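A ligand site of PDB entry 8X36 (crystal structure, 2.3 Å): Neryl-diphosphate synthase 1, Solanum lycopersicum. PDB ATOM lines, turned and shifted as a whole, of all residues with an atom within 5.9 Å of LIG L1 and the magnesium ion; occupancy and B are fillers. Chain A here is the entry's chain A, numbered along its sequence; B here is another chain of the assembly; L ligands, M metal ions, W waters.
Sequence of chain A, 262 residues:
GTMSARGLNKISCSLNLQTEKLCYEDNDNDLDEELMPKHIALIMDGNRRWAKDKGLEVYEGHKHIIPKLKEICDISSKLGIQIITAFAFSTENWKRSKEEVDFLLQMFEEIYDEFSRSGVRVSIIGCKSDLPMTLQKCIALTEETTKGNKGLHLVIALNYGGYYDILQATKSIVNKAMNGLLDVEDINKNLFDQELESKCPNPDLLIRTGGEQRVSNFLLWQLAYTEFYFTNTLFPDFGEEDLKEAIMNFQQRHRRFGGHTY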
ATOM      1  N   MET A  44      30.763 -31.512 -30.043  1.00  0.00           N
ATOM      2  CA  MET A  44      30.161 -32.168 -28.869  1.00  0.00           C
ATOM      3  C   MET A  44      28.669 -32.369 -29.090  1.00  0.00           C
ATOM      4  O   MET A  44      27.841 -31.708 -28.487  1.00  0.00           O
ATOM      5  CB  MET A  44      30.394 -31.317 -27.603  1.00  0.00           C
ATOM      6  CG  MET A  44      31.765 -30.680 -27.528  1.00  0.00           C
ATOM      7  SD  MET A  44      32.132 -29.834 -25.973  1.00  0.00           S
ATOM      8  CE  MET A  44      31.543 -28.188 -26.347  1.00  0.00           C
ATOM      9  N   ASP A  45      28.334 -33.311 -29.967  1.00  0.00           N
ATOM     10  CA  ASP A  45      26.966 -33.550 -30.420  1.00  0.00           C
ATOM     11  C   ASP A  45      26.393 -34.764 -29.690  1.00  0.00           C
ATOM     12  O   ASP A  45      27.137 -35.664 -29.273  1.00  0.00           O
ATOM     13  CB  ASP A  45      26.933 -33.772 -31.938  1.00  0.00           C
ATOM     14  CG  ASP A  45      25.531 -33.697 -32.535  1.00  0.00           C
ATOM     15  OD1 ASP A  45      24.678 -33.003 -31.949  1.00  0.00           O
ATOM     16  OD2 ASP A  45      25.293 -34.320 -33.602  1.00  0.00           O
ATOM     17  N   GLY A  46      25.077 -34.786 -29.541  1.00  0.00           N
ATOM     18  CA  GLY A  46      24.350 -35.947 -29.060  1.00  0.00           C
ATOM     19  C   GLY A  46      23.680 -35.782 -27.694  1.00  0.00           C
ATOM     20  O   GLY A  46      23.234 -36.789 -27.116  1.00  0.00           O
ATOM     21  N   ASN A  47      23.578 -34.553 -27.172  1.00  0.00           N
ATOM     22  CA  ASN A  47      23.148 -34.368 -25.795  1.00  0.00           C
ATOM     23  C   ASN A  47      21.651 -34.587 -25.605  1.00  0.00           C
ATOM     24  O   ASN A  47      21.238 -35.133 -24.583  1.00  0.00           O
ATOM     25  CB  ASN A  47      23.548 -32.973 -25.317  1.00  0.00           C
ATOM     26  CG  ASN A  47      25.039 -32.757 -25.412  1.00  0.00           C
ATOM     27  OD1 ASN A  47      25.817 -33.402 -24.713  1.00  0.00           O
ATOM     28  ND2 ASN A  47      25.455 -31.875 -26.296  1.00  0.00           N
ATOM     29  N   ARG A  48      20.818 -34.152 -26.554  1.00  0.00           N
ATOM     30  CA  ARG A  48      19.380 -34.324 -26.382  1.00  0.00           C
ATOM     31  C   ARG A  48      18.981 -35.803 -26.453  1.00  0.00           C
ATOM     32  O   ARG A  48      18.254 -36.302 -25.588  1.00  0.00           O
ATOM     33  CB  ARG A  48      18.606 -33.480 -27.417  1.00  0.00           C
ATOM     34  CG  ARG A  48      19.107 -32.023 -27.465  1.00  0.00           C
ATOM     35  CD  ARG A  48      18.192 -30.992 -28.203  1.00  0.00           C
ATOM     36  NE  ARG A  48      18.179 -31.176 -29.651  1.00  0.00           N
ATOM     37  CZ  ARG A  48      17.680 -30.321 -30.539  1.00  0.00           C
ATOM     38  NH1 ARG A  48      17.171 -29.153 -30.168  1.00  0.00           N
ATOM     39  NH2 ARG A  48      17.688 -30.643 -31.827  1.00  0.00           N
ATOM     40  N   ARG A  49      19.480 -36.532 -27.472  1.00  0.00           N
ATOM     41  CA  ARG A  49      19.172 -37.957 -27.586  1.00  0.00           C
ATOM     42  C   ARG A  49      19.670 -38.739 -26.374  1.00  0.00           C
ATOM     43  O   ARG A  49      19.048 -39.720 -25.973  1.00  0.00           O
ATOM     44  CB  ARG A  49      19.768 -38.549 -28.871  1.00  0.00           C
ATOM     45  CG  ARG A  49      19.105 -38.055 -30.165  1.00  0.00           C
ATOM     46  CD  ARG A  49      20.022 -38.241 -31.405  1.00  0.00           C
ATOM     47  NE  ARG A  49      21.097 -37.255 -31.530  1.00  0.00           N
ATOM     48  CZ  ARG A  49      22.161 -37.424 -32.321  1.00  0.00           C
ATOM     49  NH1 ARG A  49      22.349 -38.544 -32.995  1.00  0.00           N
ATOM     50  NH2 ARG A  49      23.033 -36.425 -32.461  1.00  0.00           N
ATOM     51  N   TRP A  50      20.818 -38.352 -25.814  1.00  0.00           N
ATOM     52  CA  TRP A  50      21.289 -39.015 -24.611  1.00  0.00           C
ATOM     53  C   TRP A  50      20.276 -38.868 -23.497  1.00  0.00           C
ATOM     54  O   TRP A  50      19.902 -39.845 -22.841  1.00  0.00           O
ATOM     55  CB  TRP A  50      22.631 -38.446 -24.172  1.00  0.00           C
ATOM     56  CG  TRP A  50      23.244 -39.112 -22.993  1.00  0.00           C
ATOM     57  CD1 TRP A  50      24.159 -40.128 -23.009  1.00  0.00           C
ATOM     58  CD2 TRP A  50      23.027 -38.784 -21.602  1.00  0.00           C
ATOM     59  NE1 TRP A  50      24.520 -40.449 -21.720  1.00  0.00           N
ATOM     60  CE2 TRP A  50      23.847 -39.641 -20.840  1.00  0.00           C
ATOM     61  CE3 TRP A  50      22.239 -37.846 -20.933  1.00  0.00           C
ATOM     62  CZ2 TRP A  50      23.888 -39.604 -19.439  1.00  0.00           C
ATOM     63  CZ3 TRP A  50      22.269 -37.816 -19.529  1.00  0.00           C
ATOM     64  CH2 TRP A  50      23.094 -38.685 -18.805  1.00  0.00           C
ATOM     65  N   HIS A  62      22.336 -31.317 -21.499  1.00  0.00           N
ATOM     66  CA  HIS A  62      23.208 -30.165 -21.659  1.00  0.00           C
ATOM     67  C   HIS A  62      24.031 -29.868 -20.418  1.00  0.00           C
ATOM     68  O   HIS A  62      25.117 -29.283 -20.530  1.00  0.00           O
ATOM     69  CB  HIS A  62      22.367 -28.956 -22.026  1.00  0.00           C
ATOM     70  CG  HIS A  62      21.753 -29.052 -23.384  1.00  0.00           C
ATOM     71  ND1 HIS A  62      20.481 -28.617 -23.675  1.00  0.00           N
ATOM     72  CD2 HIS A  62      22.256 -29.530 -24.555  1.00  0.00           C
ATOM     73  CE1 HIS A  62      20.219 -28.809 -24.949  1.00  0.00           C
ATOM     74  NE2 HIS A  62      21.287 -29.356 -25.513  1.00  0.00           N
ATOM     75  N   ILE A  65      27.741 -30.987 -20.543  1.00  0.00           N
ATOM     76  CA  ILE A  65      28.671 -30.506 -21.558  1.00  0.00           C
ATOM     77  C   ILE A  65      29.951 -29.988 -20.933  1.00  0.00           C
ATOM     78  O   ILE A  65      31.059 -30.443 -21.255  1.00  0.00           O
ATOM     79  CB  ILE A  65      28.002 -29.438 -22.445  1.00  0.00           C
ATOM     80  CG1 ILE A  65      26.956 -30.095 -23.359  1.00  0.00           C
ATOM     81  CG2 ILE A  65      29.056 -28.658 -23.221  1.00  0.00           C
ATOM     82  CD1 ILE A  65      26.202 -29.143 -24.226  1.00  0.00           C
ATOM     83  N   PHE A  87      33.257 -27.161 -30.108  1.00  0.00           N
ATOM     84  CA  PHE A  87      32.094 -26.481 -30.653  1.00  0.00           C
ATOM     85  C   PHE A  87      30.981 -26.515 -29.604  1.00  0.00           C
ATOM     86  O   PHE A  87      30.436 -27.588 -29.322  1.00  0.00           O
ATOM     87  CB  PHE A  87      31.694 -27.144 -31.963  1.00  0.00           C
ATOM     88  CG  PHE A  87      31.027 -26.232 -32.985  1.00  0.00           C
ATOM     89  CD1 PHE A  87      31.010 -24.856 -32.814  1.00  0.00           C
ATOM     90  CD2 PHE A  87      30.515 -26.771 -34.161  1.00  0.00           C
ATOM     91  CE1 PHE A  87      30.420 -24.028 -33.779  1.00  0.00           C
ATOM     92  CE2 PHE A  87      29.930 -25.962 -35.153  1.00  0.00           C
ATOM     93  CZ  PHE A  87      29.882 -24.589 -34.978  1.00  0.00           C
ATOM     94  N   ALA A  88      30.680 -25.378 -28.986  1.00  0.00           N
ATOM     95  CA  ALA A  88      29.684 -25.343 -27.916  1.00  0.00           C
ATOM     96  C   ALA A  88      28.340 -24.770 -28.362  1.00  0.00           C
ATOM     97  O   ALA A  88      27.311 -25.135 -27.784  1.00  0.00           O
ATOM     98  CB  ALA A  88      30.184 -24.519 -26.712  1.00  0.00           C
ATOM     99  N   PHE A  89      28.333 -23.883 -29.360  1.00  0.00           N
ATOM    100  CA  PHE A  89      27.109 -23.227 -29.809  1.00  0.00           C
ATOM    101  C   PHE A  89      27.416 -22.621 -31.169  1.00  0.00           C
ATOM    102  O   PHE A  89      28.383 -21.866 -31.284  1.00  0.00           O
ATOM    103  CB  PHE A  89      26.694 -22.136 -28.802  1.00  0.00           C
ATOM    104  CG  PHE A  89      25.289 -21.617 -28.998  1.00  0.00           C
ATOM    105  CD1 PHE A  89      24.189 -22.273 -28.449  1.00  0.00           C
ATOM    106  CD2 PHE A  89      25.081 -20.472 -29.755  1.00  0.00           C
ATOM    107  CE1 PHE A  89      22.883 -21.771 -28.640  1.00  0.00           C
ATOM    108  CE2 PHE A  89      23.794 -19.974 -29.946  1.00  0.00           C
ATOM    109  CZ  PHE A  89      22.696 -20.621 -29.400  1.00  0.00           C
ATOM    110  N   ASN A  93      22.334 -22.431 -34.099  1.00  0.00           N
ATOM    111  CA  ASN A  93      21.567 -22.932 -32.970  1.00  0.00           C
ATOM    112  C   ASN A  93      20.564 -21.910 -32.447  1.00  0.00           C
ATOM    113  O   ASN A  93      19.699 -22.275 -31.647  1.00  0.00           O
ATOM    114  CB  ASN A  93      22.501 -23.412 -31.853  1.00  0.00           C
ATOM    115  CG  ASN A  93      23.286 -24.674 -32.257  1.00  0.00           C
ATOM    116  OD1 ASN A  93      24.417 -24.890 -31.814  1.00  0.00           O
ATOM    117  ND2 ASN A  93      22.679 -25.503 -33.107  1.00  0.00           N
ATOM    118  N   ARG A  96      16.688 -22.932 -32.403  1.00  0.00           N
ATOM    119  CA  ARG A  96      15.971 -23.755 -31.442  1.00  0.00           C
ATOM    120  C   ARG A  96      15.006 -22.857 -30.661  1.00  0.00           C
ATOM    121  O   ARG A  96      14.894 -21.656 -30.901  1.00  0.00           O
ATOM    122  CB  ARG A  96      16.972 -24.500 -30.572  1.00  0.00           C
ATOM    123  CG  ARG A  96      17.866 -25.383 -31.423  1.00  0.00           C
ATOM    124  CD  ARG A  96      19.016 -25.969 -30.674  1.00  0.00           C
ATOM    125  NE  ARG A  96      19.782 -26.885 -31.503  1.00  0.00           N
ATOM    126  CZ  ARG A  96      20.541 -27.872 -31.043  1.00  0.00           C
ATOM    127  NH1 ARG A  96      20.646 -28.098 -29.743  1.00  0.00           N
ATOM    128  NH2 ARG A  96      21.200 -28.648 -31.899  1.00  0.00           N
ATOM    129  N   GLU A 100      15.062 -23.247 -25.024  1.00  0.00           N
ATOM    130  CA  GLU A 100      16.302 -24.011 -25.089  1.00  0.00           C
ATOM    131  C   GLU A 100      17.510 -23.080 -25.203  1.00  0.00           C
ATOM    132  O   GLU A 100      18.530 -23.285 -24.543  1.00  0.00           O
ATOM    133  CB  GLU A 100      16.256 -25.023 -26.237  1.00  0.00           C
ATOM    134  CG  GLU A 100      17.405 -26.022 -26.146  1.00  0.00           C
ATOM    135  CD  GLU A 100      17.521 -26.925 -27.360  1.00  0.00           C
ATOM    136  OE1 GLU A 100      16.513 -27.097 -28.075  1.00  0.00           O
ATOM    137  OE2 GLU A 100      18.628 -27.457 -27.589  1.00  0.00           O
ATOM    138  N   LEU A 104      20.686 -22.513 -22.420  1.00  0.00           N
ATOM    139  CA  LEU A 104      22.070 -22.760 -22.795  1.00  0.00           C
ATOM    140  C   LEU A 104      22.946 -21.526 -22.561  1.00  0.00           C
ATOM    141  O   LEU A 104      24.044 -21.630 -22.010  1.00  0.00           O
ATOM    142  CB  LEU A 104      22.148 -23.198 -24.256  1.00  0.00           C
ATOM    143  CG  LEU A 104      21.716 -24.653 -24.486  1.00  0.00           C
ATOM    144  CD1 LEU A 104      21.358 -24.878 -25.939  1.00  0.00           C
ATOM    145  CD2 LEU A 104      22.783 -25.628 -24.039  1.00  0.00           C
ATOM    146  N   PHE A 108      26.028 -21.500 -19.883  1.00  0.00           N
ATOM    147  CA  PHE A 108      27.433 -21.345 -20.244  1.00  0.00           C
ATOM    148  C   PHE A 108      28.185 -20.432 -19.297  1.00  0.00           C
ATOM    149  O   PHE A 108      29.421 -20.369 -19.356  1.00  0.00           O
ATOM    150  CB  PHE A 108      27.544 -20.876 -21.694  1.00  0.00           C
ATOM    151  CG  PHE A 108      27.323 -21.981 -22.695  1.00  0.00           C
ATOM    152  CD1 PHE A 108      27.935 -23.217 -22.537  1.00  0.00           C
ATOM    153  CD2 PHE A 108      26.473 -21.799 -23.761  1.00  0.00           C
ATOM    154  CE1 PHE A 108      27.726 -24.232 -23.439  1.00  0.00           C
ATOM    155  CE2 PHE A 108      26.263 -22.819 -24.682  1.00  0.00           C
ATOM    156  CZ  PHE A 108      26.887 -24.045 -24.518  1.00  0.00           C
ATOM    157  N   ARG A 208      33.963 -36.066 -33.925  1.00  0.00           N
ATOM    158  CA  ARG A 208      32.556 -35.735 -33.788  1.00  0.00           C
ATOM    159  C   ARG A 208      31.812 -36.908 -33.178  1.00  0.00           C
ATOM    160  O   ARG A 208      31.718 -37.972 -33.807  1.00  0.00           O
ATOM    161  CB  ARG A 208      31.901 -35.346 -35.108  1.00  0.00           C
ATOM    162  CG  ARG A 208      30.361 -35.211 -34.967  1.00  0.00           C
ATOM    163  CD  ARG A 208      29.702 -34.474 -36.151  1.00  0.00           C
ATOM    164  NE  ARG A 208      28.358 -34.031 -35.801  1.00  0.00           N
ATOM    165  CZ  ARG A 208      27.738 -32.992 -36.352  1.00  0.00           C
ATOM    166  NH1 ARG A 208      28.322 -32.277 -37.302  1.00  0.00           N
ATOM    167  NH2 ARG A 208      26.519 -32.655 -35.924  1.00  0.00           N
ATOM    168  N   ARG B 256      19.489 -31.637 -39.806  1.00  0.00           N
ATOM    169  CA  ARG B 256      18.827 -30.676 -38.937  1.00  0.00           C
ATOM    170  C   ARG B 256      19.248 -29.221 -39.154  1.00  0.00           C
ATOM    171  O   ARG B 256      18.487 -28.322 -38.821  1.00  0.00           O
ATOM    172  CB  ARG B 256      19.017 -31.077 -37.454  1.00  0.00           C
ATOM    173  CG  ARG B 256      18.338 -32.463 -37.135  1.00  0.00           C
ATOM    174  CD  ARG B 256      18.412 -32.930 -35.664  1.00  0.00           C
ATOM    175  NE  ARG B 256      19.612 -33.685 -35.321  1.00  0.00           N
ATOM    176  CZ  ARG B 256      19.817 -34.971 -35.567  1.00  0.00           C
ATOM    177  NH1 ARG B 256      18.900 -35.720 -36.167  1.00  0.00           N
ATOM    178  NH2 ARG B 256      20.964 -35.539 -35.197  1.00  0.00           N
HETATM  179  O1  LIG L   1      20.998 -35.335 -29.791  1.00  0.00           O
HETATM  180  P1  LIG L   1      21.088 -33.894 -30.273  1.00  0.00           P
HETATM  181  O2  LIG L   1      19.735 -33.331 -30.652  1.00  0.00           O
HETATM  182  O3  LIG L   1      22.007 -33.826 -31.477  1.00  0.00           O
HETATM  183  O4  LIG L   1      21.767 -32.992 -29.086  1.00  0.00           O
HETATM  184  P2  LIG L   1      22.437 -31.510 -29.336  1.00  0.00           P
HETATM  185  O5  LIG L   1      22.309 -31.113 -30.794  1.00  0.00           O
HETATM  186  O6  LIG L   1      21.732 -30.443 -28.533  1.00  0.00           O
HETATM  187  S1  LIG L   1      24.467 -31.631 -28.884  1.00  0.00           S
HETATM  188  C1  LIG L   1      25.275 -30.316 -29.842  1.00  0.00           C
HETATM  189  C2  LIG L   1      24.567 -29.016 -29.476  1.00  0.00           C
HETATM  190  C3  LIG L   1      25.119 -28.224 -28.570  1.00  0.00           C
HETATM  191  C4  LIG L   1      24.443 -26.922 -28.177  1.00  0.00           C
HETATM  192  C5  LIG L   1      26.445 -28.624 -27.940  1.00  0.00           C
HETATM  193  C1  LG2 L   2      26.705 -28.879 -34.059  1.00  0.00           C
HETATM  194  O1  LG2 L   2      25.655 -29.670 -33.573  1.00  0.00           O
HETATM  195  C2  LG2 L   2      26.777 -27.552 -33.301  1.00  0.00           C
HETATM  196  C3  LG2 L   2      27.343 -27.746 -31.880  1.00  0.00           C
HETATM  197  C4  LG2 L   2      27.272 -26.747 -30.998  1.00  0.00           C
HETATM  198  C5  LG2 L   2      27.999 -29.077 -31.472  1.00  0.00           C
HETATM  199  P1  LG2 L   2      24.209 -29.626 -34.344  1.00  0.00           P
HETATM  200  O2  LG2 L   2      23.200 -30.556 -33.688  1.00  0.00           O
HETATM  201  O3  LG2 L   2      23.691 -28.201 -34.406  1.00  0.00           O
HETATM  202  O4  LG2 L   2      24.482 -30.092 -35.880  1.00  0.00           O
HETATM  203  P2  LG2 L   2      23.414 -30.671 -36.978  1.00  0.00           P
HETATM  204  O5  LG2 L   2      22.121 -29.895 -36.984  1.00  0.00           O
HETATM  205  O6  LG2 L   2      23.110 -32.122 -36.670  1.00  0.00           O
HETATM  206  O7  LG2 L   2      24.114 -30.498 -38.293  1.00  0.00           O
HETATM  207 MG    MG M   1      23.059 -32.226 -32.640  1.00  0.00          MG
HETATM  208  O   HOH W   1      20.977 -31.817 -33.081  1.00  0.00           O
HETATM  209  O   HOH W   2      23.161 -33.420 -34.430  1.00  0.00           O
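The side-chain carboxylate (OD2) of Asp 45 is in salt-bridge range of the guanidinium group (NH2) of Arg 49, 3.3 Å away.
NH2 of Arg 208 lies within salt-bridge range of OD2 of Asp 45.
The backbone carbonyl oxygen (O) of Met 44 is in hydrogen-bond range of the side-chain amide nitrogen (ND2) of Asn 47 (3.2 Å).
The guanidinium group (NH1) of Arg 48 is in salt-bridge range of the side-chain carboxylate (OE1) of Glu 100, 3.0 Å away.
NH1 of Arg 96 is in salt-bridge range of OE2 of Glu 100 (3.0 Å).
The magnesium ion is bound by OD1 of Asp 45 (1.9 Å).
O2 of LG2 L2 is bound to the magnesium ion (2.0 Å).
The magnesium ion is bound by water W2 (2.2 Å).
The magnesium ion is bound by water W1 (2.2 Å).
O3 of LIG L1 binds the magnesium ion (2.2 Å).
O5 of LIG L1 binds the magnesium ion (2.3 Å).
The backbone carbonyl oxygen (O) of Met 44 lies close to a sulfur (S1) of LIG L1.
Ile 65 touches LIG L1.
O of Ala 88 touches C4 of LIG L1, 3.4 Å away.
Hydrophobic or aromatic side chains within 4 Å of LIG L1: Ile 65.
Of the 19 residues printed, 10 come within 4 Å of LIG L1.
N of Arg 49 lies within hydrogen-bond range of O1 of LIG L1, at 3.0 Å.
An oxygen (O1) of LIG L1 lies within salt-bridge range of the guanidinium group (NE) of Arg 49, 2.6 Å away.
O4 of LIG L1 sits at hydrogen-bond distance from N of Asn 47 (3.1 Å).
ND2 of Asn 47 sits close to S1 of LIG L1, at 2.8 Å.
The backbone NH (N) of Arg 48 lies within hydrogen-bond range of an oxygen (O4) of LIG L1 (2.9 Å).
The guanidinium group (NE) of Arg 48 lies within salt-bridge range of an oxygen (O2) of LIG L1 (2.8 Å).
An oxygen (O6) of LIG L1 lies within salt-bridge range of the guanidinium group of Arg 96 (2.9 Å).
An oxygen (O6) of LIG L1 sits at hydrogen-bond distance from a ring nitrogen (NE2) of His 62.
N of Gly 46 lies close to S1 of LIG L1.
NH2 of Arg 96 is in salt-bridge range of O3 of LG2 L2 (3.6 Å).
ND2 of Asn 93 sits at hydrogen-bond distance from O3 of LG2 L2, at 3.2 Å.
The guanidinium group (NH2) of Arg 208 is in salt-bridge range of an oxygen (O6) of LG2 L2, 3.5 Å away.
Water W2 lies within hydrogen-bond range of the side-chain carboxylate of Asp 45 (2.5 Å), an oxygen (O6) of LG2 L2 (2.6 Å) and the guanidinium group of Arg 256 of chain B (3.1 Å).
Water W1 lies within hydrogen-bond range of O2 of LIG L1, NE of Arg 256 of chain B and NH2 of Arg 96.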
